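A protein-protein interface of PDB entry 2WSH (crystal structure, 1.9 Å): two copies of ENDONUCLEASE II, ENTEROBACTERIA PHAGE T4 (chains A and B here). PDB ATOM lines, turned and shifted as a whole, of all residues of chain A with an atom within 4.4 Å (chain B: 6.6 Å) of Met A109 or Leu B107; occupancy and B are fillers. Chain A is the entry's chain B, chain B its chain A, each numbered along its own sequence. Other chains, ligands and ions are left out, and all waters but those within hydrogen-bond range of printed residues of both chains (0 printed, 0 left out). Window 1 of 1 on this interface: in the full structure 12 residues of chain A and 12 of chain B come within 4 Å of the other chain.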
ATOM      1  N   SER A 108     -11.172   7.414   5.410  1.00  0.00           N
ATOM      2  CA  SER A 108     -12.499   6.844   5.562  1.00  0.00           C
ATOM      3  C   SER A 108     -13.398   7.207   4.392  1.00  0.00           C
ATOM      4  O   SER A 108     -13.270   8.277   3.796  1.00  0.00           O
ATOM      5  CB  SER A 108     -13.135   7.294   6.880  1.00  0.00           C
ATOM      6  OG  SER A 108     -13.146   8.707   6.979  1.00  0.00           O
ATOM      7  N   MET A 109     -14.298   6.293   4.055  1.00  0.00           N
ATOM      8  CA  MET A 109     -15.346   6.583   3.097  1.00  0.00           C
ATOM      9  C   MET A 109     -16.679   6.257   3.741  1.00  0.00           C
ATOM     10  O   MET A 109     -16.837   5.212   4.369  1.00  0.00           O
ATOM     11  CB  MET A 109     -15.154   5.788   1.804  1.00  0.00           C
ATOM     12  CG  MET A 109     -15.230   4.282   1.961  1.00  0.00           C
ATOM     13  SD  MET A 109     -15.187   3.390   0.225  1.00  0.00           S
ATOM     14  CE  MET A 109     -16.308   4.651  -0.752  1.00  0.00           C
ATOM     15  N   THR A 110     -17.631   7.171   3.612  1.00  0.00           N
ATOM     16  CA  THR A 110     -18.966   6.931   4.126  1.00  0.00           C
ATOM     17  C   THR A 110     -19.963   6.948   2.982  1.00  0.00           C
ATOM     18  O   THR A 110     -20.160   7.975   2.330  1.00  0.00           O
ATOM     19  CB  THR A 110     -19.372   7.991   5.164  1.00  0.00           C
ATOM     20  OG1 THR A 110     -18.459   7.951   6.269  1.00  0.00           O
ATOM     21  CG2 THR A 110     -20.790   7.728   5.667  1.00  0.00           C
ATOM     22  N   ASN A 111     -20.571   5.798   2.728  1.00  0.00           N
ATOM     23  CA  ASN A 111     -21.654   5.702   1.759  1.00  0.00           C
ATOM     24  C   ASN A 111     -22.899   5.143   2.438  1.00  0.00           C
ATOM     25  O   ASN A 111     -23.015   5.200   3.662  1.00  0.00           O
ATOM     26  CB  ASN A 111     -21.242   4.854   0.548  1.00  0.00           C
ATOM     27  CG  ASN A 111     -20.873   3.434   0.926  1.00  0.00           C
ATOM     28  OD1 ASN A 111     -21.137   2.984   2.042  1.00  0.00           O
ATOM     29  ND2 ASN A 111     -20.259   2.716  -0.009  1.00  0.00           N
ATOM     30  N   GLY A 114     -22.591   2.848   5.486  1.00  0.00           N
ATOM     31  CA  GLY A 114     -21.973   3.329   6.708  1.00  0.00           C
ATOM     32  C   GLY A 114     -20.566   3.820   6.431  1.00  0.00           C
ATOM     33  O   GLY A 114     -20.269   4.271   5.327  1.00  0.00           O
ATOM     34  N   THR A 115     -19.693   3.728   7.427  1.00  0.00           N
ATOM     35  CA  THR A 115     -18.324   4.218   7.281  1.00  0.00           C
ATOM     36  C   THR A 115     -17.292   3.091   7.230  1.00  0.00           C
ATOM     37  O   THR A 115     -17.225   2.265   8.139  1.00  0.00           O
ATOM     38  CB  THR A 115     -17.956   5.173   8.424  1.00  0.00           C
ATOM     39  OG1 THR A 115     -18.731   6.373   8.315  1.00  0.00           O
ATOM     40  CG2 THR A 115     -16.472   5.524   8.374  1.00  0.00           C
ATOM     41  N   MET A 116     -16.492   3.060   6.165  1.00  0.00           N
ATOM     42  CA  MET A 116     -15.351   2.153   6.094  1.00  0.00           C
ATOM     43  C   MET A 116     -14.074   2.944   6.332  1.00  0.00           C
ATOM     44  O   MET A 116     -13.836   3.954   5.674  1.00  0.00           O
ATOM     45  CB  MET A 116     -15.255   1.452   4.735  1.00  0.00           C
ATOM     46  CG  MET A 116     -16.291   0.367   4.474  1.00  0.00           C
ATOM     47  SD  MET A 116     -17.566   0.883   3.090  1.00  0.00           S
ATOM     48  CE  MET A 116     -18.516   2.198   4.109  1.00  0.00           C
ATOM     49  N   PHE B 105     -16.116   0.728  -7.312  1.00  0.00           N
ATOM     50  CA  PHE B 105     -14.980   1.398  -7.931  1.00  0.00           C
ATOM     51  C   PHE B 105     -13.674   1.014  -7.254  1.00  0.00           C
ATOM     52  O   PHE B 105     -13.633   0.105  -6.423  1.00  0.00           O
ATOM     53  CB  PHE B 105     -15.170   2.912  -7.859  1.00  0.00           C
ATOM     54  CG  PHE B 105     -15.342   3.425  -6.463  1.00  0.00           C
ATOM     55  CD1 PHE B 105     -14.279   3.998  -5.787  1.00  0.00           C
ATOM     56  CD2 PHE B 105     -16.559   3.310  -5.816  1.00  0.00           C
ATOM     57  CE1 PHE B 105     -14.431   4.461  -4.498  1.00  0.00           C
ATOM     58  CE2 PHE B 105     -16.718   3.771  -4.528  1.00  0.00           C
ATOM     59  CZ  PHE B 105     -15.651   4.346  -3.869  1.00  0.00           C
ATOM     60  N   ASN B 106     -12.605   1.716  -7.609  1.00  0.00           N
ATOM     61  CA  ASN B 106     -11.296   1.451  -7.027  1.00  0.00           C
ATOM     62  C   ASN B 106     -10.684   2.667  -6.346  1.00  0.00           C
ATOM     63  O   ASN B 106     -10.876   3.801  -6.781  1.00  0.00           O
ATOM     64  CB  ASN B 106     -10.350   0.896  -8.092  1.00  0.00           C
ATOM     65  CG  ASN B 106     -10.727  -0.506  -8.522  1.00  0.00           C
ATOM     66  OD1 ASN B 106     -10.403  -1.482  -7.847  1.00  0.00           O
ATOM     67  ND2 ASN B 106     -11.422  -0.612  -9.646  1.00  0.00           N
ATOM     68  N   LEU B 107      -9.956   2.420  -5.265  1.00  0.00           N
ATOM     69  CA  LEU B 107      -9.252   3.476  -4.556  1.00  0.00           C
ATOM     70  C   LEU B 107      -7.768   3.142  -4.500  1.00  0.00           C
ATOM     71  O   LEU B 107      -7.387   2.004  -4.221  1.00  0.00           O
ATOM     72  CB  LEU B 107      -9.816   3.642  -3.145  1.00  0.00           C
ATOM     73  CG  LEU B 107     -11.244   4.183  -3.076  1.00  0.00           C
ATOM     74  CD1 LEU B 107     -11.843   3.955  -1.696  1.00  0.00           C
ATOM     75  CD2 LEU B 107     -11.253   5.656  -3.428  1.00  0.00           C
ATOM     76  N   SER B 108      -6.937   4.134  -4.781  1.00  0.00           N
ATOM     77  CA  SER B 108      -5.498   3.936  -4.782  1.00  0.00           C
ATOM     78  C   SER B 108      -4.800   5.023  -3.992  1.00  0.00           C
ATOM     79  O   SER B 108      -5.252   6.165  -3.944  1.00  0.00           O
ATOM     80  CB  SER B 108      -4.953   3.902  -6.208  1.00  0.00           C
ATOM     81  OG  SER B 108      -5.210   2.645  -6.809  1.00  0.00           O
ATOM     82  N   MET B 109      -3.692   4.647  -3.369  1.00  0.00           N
ATOM     83  CA  MET B 109      -2.868   5.582  -2.629  1.00  0.00           C
ATOM     84  C   MET B 109      -1.430   5.337  -3.033  1.00  0.00           C
ATOM     85  O   MET B 109      -1.000   4.191  -3.140  1.00  0.00           O
ATOM     86  CB  MET B 109      -3.042   5.360  -1.131  1.00  0.00           C
ATOM     87  CG  MET B 109      -1.964   5.974  -0.273  1.00  0.00           C
ATOM     88  SD  MET B 109      -2.111   5.309   1.556  1.00  0.00           S
ATOM     89  CE  MET B 109      -0.365   5.886   2.208  1.00  0.00           C
ATOM     90  N   MET B 116      -0.738   1.383  -3.128  1.00  0.00           N
ATOM     91  CA  MET B 116      -1.681   0.489  -2.472  1.00  0.00           C
ATOM     92  C   MET B 116      -3.055   0.715  -3.088  1.00  0.00           C
ATOM     93  O   MET B 116      -3.446   1.856  -3.331  1.00  0.00           O
ATOM     94  CB  MET B 116      -1.742   0.769  -0.968  1.00  0.00           C
ATOM     95  CG  MET B 116      -0.513   0.336  -0.160  1.00  0.00           C
ATOM     96  SD  MET B 116       0.646   1.807   0.433  1.00  0.00           S
ATOM     97  CE  MET B 116       1.533   2.122  -1.238  1.00  0.00           C
ATOM     98  N   THR B 117      -3.789  -0.365  -3.332  1.00  0.00           N
ATOM     99  CA  THR B 117      -5.087  -0.249  -3.985  1.00  0.00           C
ATOM    100  C   THR B 117      -6.141  -1.184  -3.395  1.00  0.00           C
ATOM    101  O   THR B 117      -5.832  -2.293  -2.955  1.00  0.00           O
ATOM    102  CB  THR B 117      -4.977  -0.503  -5.500  1.00  0.00           C
ATOM    103  OG1 THR B 117      -6.280  -0.439  -6.094  1.00  0.00           O
ATOM    104  CG2 THR B 117      -4.365  -1.871  -5.766  1.00  0.00           C
ATOM    105  N   ILE B 118      -7.388  -0.722  -3.395  1.00  0.00           N
ATOM    106  CA  ILE B 118      -8.507  -1.522  -2.909  1.00  0.00           C
ATOM    107  C   ILE B 118      -9.708  -1.434  -3.848  1.00  0.00           C
ATOM    108  O   ILE B 118     -10.122  -0.343  -4.242  1.00  0.00           O
ATOM    109  CB  ILE B 118      -8.950  -1.092  -1.499  1.00  0.00           C
ATOM    110  CG1 ILE B 118     -10.101  -1.974  -1.007  1.00  0.00           C
ATOM    111  CG2 ILE B 118      -9.378   0.361  -1.488  1.00  0.00           C
ATOM    112  CD1 ILE B 118      -9.738  -3.436  -0.876  1.00  0.00           C
ATOM    113  N   ALA B 119     -10.250  -2.588  -4.224  1.00  0.00           N
ATOM    114  CA  ALA B 119     -11.519  -2.637  -4.932  1.00  0.00           C
ATOM    115  C   ALA B 119     -12.608  -2.602  -3.873  1.00  0.00           C
ATOM    116  O   ALA B 119     -12.615  -3.429  -2.962  1.00  0.00           O
ATOM    117  CB  ALA B 119     -11.619  -3.906  -5.762  1.00  0.00           C
ATOM    118  N   THR B 120     -13.521  -1.643  -3.978  1.00  0.00           N
ATOM    119  CA  THR B 120     -14.515  -1.453  -2.928  1.00  0.00           C
ATOM    120  C   THR B 120     -15.493  -2.624  -2.802  1.00  0.00           C
ATOM    121  O   THR B 120     -16.127  -2.785  -1.762  1.00  0.00           O
ATOM    122  CB  THR B 120     -15.298  -0.131  -3.089  1.00  0.00           C
ATOM    123  OG1 THR B 120     -16.044  -0.159  -4.309  1.00  0.00           O
ATOM    124  CG2 THR B 120     -14.346   1.055  -3.095  1.00  0.00           C
ATOM    125  N   LEU B 123     -14.733  -4.412   0.131  1.00  0.00           N
ATOM    126  CA  LEU B 123     -15.172  -3.766   1.365  1.00  0.00           C
ATOM    127  C   LEU B 123     -16.674  -3.906   1.586  1.00  0.00           C
ATOM    128  O   LEU B 123     -17.136  -3.988   2.722  1.00  0.00           O
ATOM    129  CB  LEU B 123     -14.832  -2.276   1.333  1.00  0.00           C
ATOM    130  CG  LEU B 123     -13.365  -1.851   1.361  1.00  0.00           C
ATOM    131  CD1 LEU B 123     -13.274  -0.332   1.272  1.00  0.00           C
ATOM    132  CD2 LEU B 123     -12.687  -2.368   2.618  1.00  0.00           C
ATOM    133  N   GLU B 124     -17.433  -3.914   0.495  1.00  0.00           N
ATOM    134  CA  GLU B 124     -18.887  -3.842   0.583  1.00  0.00           C
ATOM    135  C   GLU B 124     -19.560  -5.199   0.777  1.00  0.00           C
ATOM    136  O   GLU B 124     -20.525  -5.314   1.531  1.00  0.00           O
ATOM    137  CB  GLU B 124     -19.463  -3.139  -0.649  1.00  0.00           C
ATOM    138  CG  GLU B 124     -19.188  -1.644  -0.691  1.00  0.00           C
ATOM    139  CD  GLU B 124     -20.148  -0.900  -1.597  1.00  0.00           C
ATOM    140  OE1 GLU B 124     -20.964  -1.561  -2.272  1.00  0.00           O
ATOM    141  OE2 GLU B 124     -20.087   0.344  -1.633  1.00  0.00           O
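The side-chain carboxylate (OE2) of Glu B124 sits at hydrogen-bond distance from the side-chain amide nitrogen (ND2) of Asn A111 (2.9 Å).
N of Thr B120 lies within hydrogen-bond range of O of Phe B105 (3.0 Å). OG1 of Thr B117 sits close to O of Leu B107 (3.3 Å). The backbone carbonyl oxygen of Leu B107 sits at hydrogen-bond distance from the backbone NH of Ile B118 (2.8 Å). The backbone NH (N) of Met A116 is in hydrogen-bond range of the backbone carbonyl oxygen (O) of Met A109.
CE of Met A109 touches CZ of Phe B105, 3.2 Å away. Leu B107 touches Met A109.
Met A109 touches just these residues of chain B: Phe B105 and Leu B107. Of the printed residues of chain A, Leu B107 touches Met A109 (3.9 Å). Of the printed residues of chain A, Phe B105 touches Met A109. Of the printed residues of chain B, Asn A111 touches Glu B124. Of the printed residues of chain A, Glu B124 touches Asn A111. The nearest residue of chain B that does not touch Met A109 is Thr B120 (4.1 Å). The nearest printed residue of chain A that does not touch Leu B107 is Ser A108 (7.1 Å). The nearest printed residue of chain A that does not touch Glu B124 is Met A116 (4.8 Å).
Of the 12 printed residues of chain B, 3 touch a printed residue of chain A. Hydrophobic or aromatic side chains of chain B within 4 Å of the printed part of chain A: Phe B105 and Leu B107. Of the 7 printed residues of chain A, 2 touch a printed residue of chain B. Hydrophobic or aromatic side chains of chain A within 4 Å of the printed part of chain B: Met A109. Along chain A the printed residues that touch a printed residue of chain B span positions 109 to 111. Among the printed residues, 3 pairs touch across the chains. Among the printed residues, no Asp or Glu carboxylate lies within 4 Å of a Lys or Arg side-chain nitrogen of the other chain.
3 positions are printed for both chains.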
